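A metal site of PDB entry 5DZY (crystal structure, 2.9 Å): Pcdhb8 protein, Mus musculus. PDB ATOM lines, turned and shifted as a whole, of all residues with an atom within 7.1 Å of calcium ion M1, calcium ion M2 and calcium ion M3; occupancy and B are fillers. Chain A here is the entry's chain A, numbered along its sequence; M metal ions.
Calcium ion M1 is bound by the side-chain carboxylate (OE2) of Glu 65 (2.4 Å), the side-chain carboxylate (OD1) of Asp 100 (2.5 Å), the side-chain carboxylate (OD1) of Asp 97 (2.6 Å), the backbone carbonyl oxygen (O) of Ile 98 (2.6 Å), the side-chain carboxylate (OD1) of Asp 133 (2.8 Å) and the side-chain carboxylate (OE1) of Glu 9 (2.8 Å).
Calcium ion M2 is bound by the side-chain carboxylate (OD2) of Asp 100 (2.2 Å), the side-chain carboxylate (OD1) of Asp 63 (2.5 Å) and the side-chain carboxylate (OE1) of Glu 65 (2.7 Å).
Calcium ion M2 has three donor atoms within binding distance.
Slightly farther from calcium ion M2 lies the side-chain carboxylate (OE2) of Glu 9 (2.9 Å).
Slightly farther from calcium ion M2 lies a ring nitrogen (NE2) of His 101 (3.0 Å).
Slightly farther from calcium ion M2 lies the side-chain carboxylate (OD1) of Asp 100 (3.1 Å).
Residues that only touch calcium ion M2: Glu 10.
Of the 28 residues printed, 6 come within 4 Å of calcium ion M2.
The nearest printed residue that does not touch calcium ion M2 is Arg 64 (5.2 Å).
Calcium ion M3 is bound by the side-chain carboxylate of Asp 131 (2.2 Å), the side-chain carboxylate of Asp 188 (2.3 Å), the side-chain carboxylate of Asp 133 (2.3 Å), the backbone carbonyl oxygen of His 101 (2.5 Å), the side-chain amide oxygen of Asn 99 (2.5 Å) and the backbone carbonyl oxygen of Asn 137 (2.7 Å).
Calcium ion M3 has six donor atoms within binding distance.
Slightly farther from calcium ion M3 lies the side-chain carboxylate (OD1) of Asp 131 (2.9 Å).
Within 4 Å of calcium ion M1: Glu 9, Glu 65, Asp 97, Ile 98, Asp 100, His 101 and Asp 133.
The backbone NH (N) of Asp 188 sits at hydrogen-bond distance from the backbone carbonyl oxygen (O) of Lys 194, at 2.8 Å.
The side-chain carboxylate (OD1) of Asp 188 lies within hydrogen-bond range of the backbone NH (N) of Gly 190 (3.0 Å).
The side-chain carboxylate (OE1) of Glu 65 sits close to a ring nitrogen (NE2) of His 101 (3.4 Å).
The side-chain carboxylate (OE2) of Glu 65 sits close to the guanidinium group (NH1) of Arg 64, at 2.9 Å.
The backbone NH (N) of Ala 66 lies within hydrogen-bond range of the side-chain carboxylate (OD2) of Asp 63 (3.1 Å).
OD1 of Asp 97 lies close to NH1 of Arg 64.
The backbone NH of Glu 9 sits at hydrogen-bond distance from the backbone carbonyl oxygen of Thr 96 (2.8 Å).
The backbone carbonyl oxygen (O) of Pro 62 sits at hydrogen-bond distance from the backbone NH (N) of Glu 10 (3.2 Å).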
ATOM      1  N   GLU A   9     -32.709   7.187  15.951  1.00  0.00           N
ATOM      2  CA  GLU A   9     -31.645   7.126  14.957  1.00  0.00           C
ATOM      3  C   GLU A   9     -30.642   6.022  15.292  1.00  0.00           C
ATOM      4  O   GLU A   9     -30.531   5.595  16.435  1.00  0.00           O
ATOM      5  CB  GLU A   9     -30.930   8.481  14.877  1.00  0.00           C
ATOM      6  CG  GLU A   9     -29.914   8.609  13.749  1.00  0.00           C
ATOM      7  CD  GLU A   9     -29.011   9.819  13.915  1.00  0.00           C
ATOM      8  OE1 GLU A   9     -29.276  10.639  14.830  1.00  0.00           O
ATOM      9  OE2 GLU A   9     -28.049   9.954  13.139  1.00  0.00           O
ATOM     10  N   GLU A  10     -29.918   5.555  14.270  1.00  0.00           N
ATOM     11  CA  GLU A  10     -28.836   4.589  14.431  1.00  0.00           C
ATOM     12  C   GLU A  10     -29.284   3.285  15.071  1.00  0.00           C
ATOM     13  O   GLU A  10     -28.541   2.666  15.831  1.00  0.00           O
ATOM     14  CB  GLU A  10     -27.697   5.204  15.257  1.00  0.00           C
ATOM     15  CG  GLU A  10     -26.969   6.357  14.575  1.00  0.00           C
ATOM     16  CD  GLU A  10     -25.994   5.894  13.513  1.00  0.00           C
ATOM     17  OE1 GLU A  10     -25.822   4.669  13.346  1.00  0.00           O
ATOM     18  OE2 GLU A  10     -25.390   6.761  12.846  1.00  0.00           O
ATOM     19  N   PRO A  62     -29.798   3.439   9.576  1.00  0.00           N
ATOM     20  CA  PRO A  62     -29.997   4.837   9.168  1.00  0.00           C
ATOM     21  C   PRO A  62     -29.223   5.853  10.008  1.00  0.00           C
ATOM     22  O   PRO A  62     -29.058   5.664  11.215  1.00  0.00           O
ATOM     23  CB  PRO A  62     -31.509   5.025   9.357  1.00  0.00           C
ATOM     24  CG  PRO A  62     -31.830   4.139  10.506  1.00  0.00           C
ATOM     25  CD  PRO A  62     -30.919   2.945  10.394  1.00  0.00           C
ATOM     26  N   ASP A  63     -28.752   6.912   9.355  1.00  0.00           N
ATOM     27  CA  ASP A  63     -28.105   8.023  10.048  1.00  0.00           C
ATOM     28  C   ASP A  63     -28.764   9.329   9.638  1.00  0.00           C
ATOM     29  O   ASP A  63     -28.711   9.723   8.473  1.00  0.00           O
ATOM     30  CB  ASP A  63     -26.612   8.055   9.725  1.00  0.00           C
ATOM     31  CG  ASP A  63     -25.894   9.210  10.412  1.00  0.00           C
ATOM     32  OD1 ASP A  63     -25.476   9.050  11.577  1.00  0.00           O
ATOM     33  OD2 ASP A  63     -25.754  10.277   9.772  1.00  0.00           O
ATOM     34  N   ARG A  64     -29.385   9.998  10.604  1.00  0.00           N
ATOM     35  CA  ARG A  64     -30.191  11.193  10.355  1.00  0.00           C
ATOM     36  C   ARG A  64     -29.410  12.290   9.633  1.00  0.00           C
ATOM     37  O   ARG A  64     -29.897  12.861   8.655  1.00  0.00           O
ATOM     38  CB  ARG A  64     -30.747  11.730  11.678  1.00  0.00           C
ATOM     39  CG  ARG A  64     -32.112  12.422  11.579  1.00  0.00           C
ATOM     40  CD  ARG A  64     -32.013  13.791  10.928  1.00  0.00           C
ATOM     41  NE  ARG A  64     -30.862  14.543  11.421  1.00  0.00           N
ATOM     42  CZ  ARG A  64     -30.861  15.273  12.528  1.00  0.00           C
ATOM     43  NH1 ARG A  64     -29.765  15.932  12.892  1.00  0.00           N
ATOM     44  NH2 ARG A  64     -31.951  15.354  13.274  1.00  0.00           N
ATOM     45  N   GLU A  65     -28.213  12.569  10.118  1.00  0.00           N
ATOM     46  CA  GLU A  65     -27.402  13.658   9.572  1.00  0.00           C
ATOM     47  C   GLU A  65     -27.024  13.431   8.114  1.00  0.00           C
ATOM     48  O   GLU A  65     -26.775  14.379   7.368  1.00  0.00           O
ATOM     49  CB  GLU A  65     -26.136  13.855  10.410  1.00  0.00           C
ATOM     50  CG  GLU A  65     -26.381  14.445  11.795  1.00  0.00           C
ATOM     51  CD  GLU A  65     -27.005  13.459  12.760  1.00  0.00           C
ATOM     52  OE1 GLU A  65     -26.645  12.262  12.698  1.00  0.00           O
ATOM     53  OE2 GLU A  65     -27.864  13.865  13.568  1.00  0.00           O
ATOM     54  N   ALA A  66     -26.990  12.171   7.700  1.00  0.00           N
ATOM     55  CA  ALA A  66     -26.656  11.817   6.325  1.00  0.00           C
ATOM     56  C   ALA A  66     -27.908  11.693   5.470  1.00  0.00           C
ATOM     57  O   ALA A  66     -27.833  11.677   4.234  1.00  0.00           O
ATOM     58  CB  ALA A  66     -25.853  10.530   6.286  1.00  0.00           C
ATOM     59  N   THR A  96     -36.204   9.828  14.942  1.00  0.00           N
ATOM     60  CA  THR A  96     -35.884  10.682  16.073  1.00  0.00           C
ATOM     61  C   THR A  96     -34.365  10.794  16.245  1.00  0.00           C
ATOM     62  O   THR A  96     -33.678   9.786  16.358  1.00  0.00           O
ATOM     63  CB  THR A  96     -36.502  10.164  17.383  1.00  0.00           C
ATOM     64  OG1 THR A  96     -37.932  10.207  17.276  1.00  0.00           O
ATOM     65  CG2 THR A  96     -36.069  11.014  18.565  1.00  0.00           C
ATOM     66  N   ASP A  97     -33.871  12.033  16.261  1.00  0.00           N
ATOM     67  CA  ASP A  97     -32.434  12.269  16.371  1.00  0.00           C
ATOM     68  C   ASP A  97     -31.904  11.863  17.746  1.00  0.00           C
ATOM     69  O   ASP A  97     -32.553  12.074  18.763  1.00  0.00           O
ATOM     70  CB  ASP A  97     -32.126  13.750  16.111  1.00  0.00           C
ATOM     71  CG  ASP A  97     -30.655  14.066  16.281  1.00  0.00           C
ATOM     72  OD1 ASP A  97     -29.911  14.001  15.274  1.00  0.00           O
ATOM     73  OD2 ASP A  97     -30.239  14.388  17.415  1.00  0.00           O
ATOM     74  N   ILE A  98     -30.704  11.286  17.748  1.00  0.00           N
ATOM     75  CA  ILE A  98     -30.034  10.925  18.991  1.00  0.00           C
ATOM     76  C   ILE A  98     -28.740  11.717  19.149  1.00  0.00           C
ATOM     77  O   ILE A  98     -28.215  12.262  18.176  1.00  0.00           O
ATOM     78  CB  ILE A  98     -29.712   9.413  19.051  1.00  0.00           C
ATOM     79  CG1 ILE A  98     -28.713   9.044  17.959  1.00  0.00           C
ATOM     80  CG2 ILE A  98     -30.989   8.598  18.928  1.00  0.00           C
ATOM     81  CD1 ILE A  98     -28.261   7.599  18.012  1.00  0.00           C
ATOM     82  N   ASN A  99     -28.237  11.790  20.375  1.00  0.00           N
ATOM     83  CA  ASN A  99     -26.999  12.504  20.643  1.00  0.00           C
ATOM     84  C   ASN A  99     -25.783  11.613  20.385  1.00  0.00           C
ATOM     85  O   ASN A  99     -25.131  11.159  21.330  1.00  0.00           O
ATOM     86  CB  ASN A  99     -26.979  13.031  22.081  1.00  0.00           C
ATOM     87  CG  ASN A  99     -25.815  13.964  22.351  1.00  0.00           C
ATOM     88  OD1 ASN A  99     -25.231  14.516  21.424  1.00  0.00           O
ATOM     89  ND2 ASN A  99     -25.479  14.138  23.623  1.00  0.00           N
ATOM     90  N   ASP A 100     -25.497  11.362  19.120  1.00  0.00           N
ATOM     91  CA  ASP A 100     -24.389  10.485  18.739  1.00  0.00           C
ATOM     92  C   ASP A 100     -23.253  11.258  18.083  1.00  0.00           C
ATOM     93  O   ASP A 100     -22.427  10.678  17.372  1.00  0.00           O
ATOM     94  CB  ASP A 100     -24.893   9.378  17.815  1.00  0.00           C
ATOM     95  CG  ASP A 100     -25.585   9.925  16.574  1.00  0.00           C
ATOM     96  OD1 ASP A 100     -26.016  11.094  16.594  1.00  0.00           O
ATOM     97  OD2 ASP A 100     -25.702   9.175  15.587  1.00  0.00           O
ATOM     98  N   HIS A 101     -23.216  12.564  18.312  1.00  0.00           N
ATOM     99  CA  HIS A 101     -22.153  13.414  17.779  1.00  0.00           C
ATOM    100  C   HIS A 101     -21.491  14.221  18.883  1.00  0.00           C
ATOM    101  O   HIS A 101     -22.173  14.911  19.655  1.00  0.00           O
ATOM    102  CB  HIS A 101     -22.692  14.341  16.694  1.00  0.00           C
ATOM    103  CG  HIS A 101     -22.804  13.705  15.344  1.00  0.00           C
ATOM    104  ND1 HIS A 101     -21.815  13.787  14.390  1.00  0.00           N
ATOM    105  CD2 HIS A 101     -23.799  12.963  14.791  1.00  0.00           C
ATOM    106  CE1 HIS A 101     -22.191  13.126  13.306  1.00  0.00           C
ATOM    107  NE2 HIS A 101     -23.389  12.621  13.526  1.00  0.00           N
ATOM    108  N   PHE A 102     -20.168  14.139  18.976  1.00  0.00           N
ATOM    109  CA  PHE A 102     -19.417  14.925  19.946  1.00  0.00           C
ATOM    110  C   PHE A 102     -19.130  16.322  19.402  1.00  0.00           C
ATOM    111  O   PHE A 102     -18.786  16.470  18.235  1.00  0.00           O
ATOM    112  CB  PHE A 102     -18.109  14.222  20.317  1.00  0.00           C
ATOM    113  CG  PHE A 102     -18.289  13.021  21.197  1.00  0.00           C
ATOM    114  CD1 PHE A 102     -19.489  12.794  21.854  1.00  0.00           C
ATOM    115  CD2 PHE A 102     -17.247  12.121  21.380  1.00  0.00           C
ATOM    116  CE1 PHE A 102     -19.649  11.690  22.672  1.00  0.00           C
ATOM    117  CE2 PHE A 102     -17.408  11.016  22.198  1.00  0.00           C
ATOM    118  CZ  PHE A 102     -18.611  10.809  22.842  1.00  0.00           C
ATOM    119  N   PRO A 103     -19.270  17.342  20.261  1.00  0.00           N
ATOM    120  CA  PRO A 103     -18.936  18.722  19.891  1.00  0.00           C
ATOM    121  C   PRO A 103     -17.475  18.841  19.450  1.00  0.00           C
ATOM    122  O   PRO A 103     -16.577  18.440  20.192  1.00  0.00           O
ATOM    123  CB  PRO A 103     -19.183  19.506  21.185  1.00  0.00           C
ATOM    124  CG  PRO A 103     -20.177  18.684  21.931  1.00  0.00           C
ATOM    125  CD  PRO A 103     -19.834  17.255  21.617  1.00  0.00           C
ATOM    126  N   GLN A 130     -19.129  23.175  16.830  1.00  0.00           N
ATOM    127  CA  GLN A 130     -20.211  22.744  15.942  1.00  0.00           C
ATOM    128  C   GLN A 130     -20.725  21.356  16.308  1.00  0.00           C
ATOM    129  O   GLN A 130     -19.971  20.494  16.759  1.00  0.00           O
ATOM    130  CB  GLN A 130     -19.734  22.772  14.490  1.00  0.00           C
ATOM    131  CG  GLN A 130     -19.384  24.164  13.986  1.00  0.00           C
ATOM    132  CD  GLN A 130     -18.896  24.165  12.556  1.00  0.00           C
ATOM    133  OE1 GLN A 130     -18.530  23.125  12.009  1.00  0.00           O
ATOM    134  NE2 GLN A 130     -18.873  25.345  11.945  1.00  0.00           N
ATOM    135  N   ASP A 131     -22.023  21.152  16.104  1.00  0.00           N
ATOM    136  CA  ASP A 131     -22.660  19.876  16.414  1.00  0.00           C
ATOM    137  C   ASP A 131     -23.787  19.605  15.433  1.00  0.00           C
ATOM    138  O   ASP A 131     -24.799  20.315  15.416  1.00  0.00           O
ATOM    139  CB  ASP A 131     -23.197  19.891  17.849  1.00  0.00           C
ATOM    140  CG  ASP A 131     -23.362  18.492  18.425  1.00  0.00           C
ATOM    141  OD1 ASP A 131     -23.636  17.557  17.648  1.00  0.00           O
ATOM    142  OD2 ASP A 131     -23.221  18.336  19.654  1.00  0.00           O
ATOM    143  N   PRO A 132     -23.621  18.560  14.598  1.00  0.00           N
ATOM    144  CA  PRO A 132     -24.573  18.192  13.541  1.00  0.00           C
ATOM    145  C   PRO A 132     -25.950  17.781  14.059  1.00  0.00           C
ATOM    146  O   PRO A 132     -26.870  17.588  13.255  1.00  0.00           O
ATOM    147  CB  PRO A 132     -23.889  17.003  12.847  1.00  0.00           C
ATOM    148  CG  PRO A 132     -22.445  17.151  13.191  1.00  0.00           C
ATOM    149  CD  PRO A 132     -22.419  17.708  14.566  1.00  0.00           C
ATOM    150  N   ASP A 133     -26.097  17.641  15.377  1.00  0.00           N
ATOM    151  CA  ASP A 133     -27.356  17.228  15.969  1.00  0.00           C
ATOM    152  C   ASP A 133     -28.407  18.333  15.921  1.00  0.00           C
ATOM    153  O   ASP A 133     -28.157  19.417  15.383  1.00  0.00           O
ATOM    154  CB  ASP A 133     -27.145  16.789  17.416  1.00  0.00           C
ATOM    155  CG  ASP A 133     -26.125  15.663  17.542  1.00  0.00           C
ATOM    156  OD1 ASP A 133     -25.988  14.881  16.576  1.00  0.00           O
ATOM    157  OD2 ASP A 133     -25.467  15.575  18.595  1.00  0.00           O
ATOM    158  N   ILE A 134     -29.581  18.063  16.479  1.00  0.00           N
ATOM    159  CA  ILE A 134     -30.692  19.014  16.451  1.00  0.00           C
ATOM    160  C   ILE A 134     -31.361  19.152  17.813  1.00  0.00           C
ATOM    161  O   ILE A 134     -31.692  18.156  18.456  1.00  0.00           O
ATOM    162  CB  ILE A 134     -31.758  18.606  15.401  1.00  0.00           C
ATOM    163  CG1 ILE A 134     -31.203  18.783  13.981  1.00  0.00           C
ATOM    164  CG2 ILE A 134     -33.028  19.412  15.575  1.00  0.00           C
ATOM    165  CD1 ILE A 134     -32.248  18.608  12.897  1.00  0.00           C
ATOM    166  N   SER A 136     -31.923  19.741  21.678  1.00  0.00           N
ATOM    167  CA  SER A 136     -31.216  19.523  22.940  1.00  0.00           C
ATOM    168  C   SER A 136     -29.958  18.686  22.734  1.00  0.00           C
ATOM    169  O   SER A 136     -29.056  18.691  23.577  1.00  0.00           O
ATOM    170  CB  SER A 136     -32.144  18.850  23.951  1.00  0.00           C
ATOM    171  OG  SER A 136     -31.476  18.653  25.188  1.00  0.00           O
ATOM    172  N   ASN A 137     -29.899  17.986  21.606  1.00  0.00           N
ATOM    173  CA  ASN A 137     -28.742  17.156  21.285  1.00  0.00           C
ATOM    174  C   ASN A 137     -27.596  17.984  20.701  1.00  0.00           C
ATOM    175  O   ASN A 137     -26.500  17.465  20.479  1.00  0.00           O
ATOM    176  CB  ASN A 137     -29.140  16.049  20.308  1.00  0.00           C
ATOM    177  CG  ASN A 137     -30.139  15.084  20.907  1.00  0.00           C
ATOM    178  OD1 ASN A 137     -30.123  14.816  22.117  1.00  0.00           O
ATOM    179  ND2 ASN A 137     -31.009  14.539  20.064  1.00  0.00           N
ATOM    180  N   ALA A 138     -27.854  19.263  20.453  1.00  0.00           N
ATOM    181  CA  ALA A 138     -26.846  20.162  19.915  1.00  0.00           C
ATOM    182  C   ALA A 138     -26.100  20.886  21.033  1.00  0.00           C
ATOM    183  O   ALA A 138     -26.247  20.549  22.208  1.00  0.00           O
ATOM    184  CB  ALA A 138     -27.480  21.164  18.963  1.00  0.00           C
ATOM    185  N   VAL A 139     -25.293  21.866  20.662  1.00  0.00           N
ATOM    186  CA  VAL A 139     -24.533  22.644  21.640  1.00  0.00           C
ATOM    187  C   VAL A 139     -25.461  23.425  22.560  1.00  0.00           C
ATOM    188  O   VAL A 139     -26.406  24.072  22.117  1.00  0.00           O
ATOM    189  CB  VAL A 139     -23.558  23.619  20.949  1.00  0.00           C
ATOM    190  CG1 VAL A 139     -22.317  22.885  20.481  1.00  0.00           C
ATOM    191  CG2 VAL A 139     -24.237  24.328  19.786  1.00  0.00           C
ATOM    192  N   ASP A 188     -22.892  19.521  25.813  1.00  0.00           N
ATOM    193  CA  ASP A 188     -24.139  19.221  25.129  1.00  0.00           C
ATOM    194  C   ASP A 188     -25.299  19.260  26.115  1.00  0.00           C
ATOM    195  O   ASP A 188     -25.098  19.197  27.324  1.00  0.00           O
ATOM    196  CB  ASP A 188     -24.048  17.849  24.443  1.00  0.00           C
ATOM    197  CG  ASP A 188     -25.109  17.640  23.379  1.00  0.00           C
ATOM    198  OD1 ASP A 188     -26.260  18.091  23.576  1.00  0.00           O
ATOM    199  OD2 ASP A 188     -24.795  17.029  22.347  1.00  0.00           O
ATOM    200  N   GLY A 189     -26.523  19.358  25.593  1.00  0.00           N
ATOM    201  CA  GLY A 189     -27.708  19.403  26.433  1.00  0.00           C
ATOM    202  C   GLY A 189     -28.399  18.061  26.538  1.00  0.00           C
ATOM    203  O   GLY A 189     -29.467  17.940  27.149  1.00  0.00           O
ATOM    204  N   GLY A 190     -27.806  17.036  25.924  1.00  0.00           N
ATOM    205  CA  GLY A 190     -28.368  15.706  25.939  1.00  0.00           C
ATOM    206  C   GLY A 190     -28.057  14.964  27.226  1.00  0.00           C
ATOM    207  O   GLY A 190     -27.373  15.476  28.110  1.00  0.00           O
ATOM    208  N   LYS A 194     -22.488  15.486  26.073  1.00  0.00           N
ATOM    209  CA  LYS A 194     -21.247  15.249  25.358  1.00  0.00           C
ATOM    210  C   LYS A 194     -20.385  16.503  25.370  1.00  0.00           C
ATOM    211  O   LYS A 194     -20.892  17.620  25.328  1.00  0.00           O
ATOM    212  CB  LYS A 194     -21.539  14.824  23.912  1.00  0.00           C
HETATM  213 CA    CA M   1     -27.678  12.808  15.720  1.00  0.00          CA
HETATM  214 CA    CA M   2     -25.192  10.275  13.708  1.00  0.00          CA
HETATM  215 CA    CA M   3     -24.072  16.372  20.261  1.00  0.00          CA
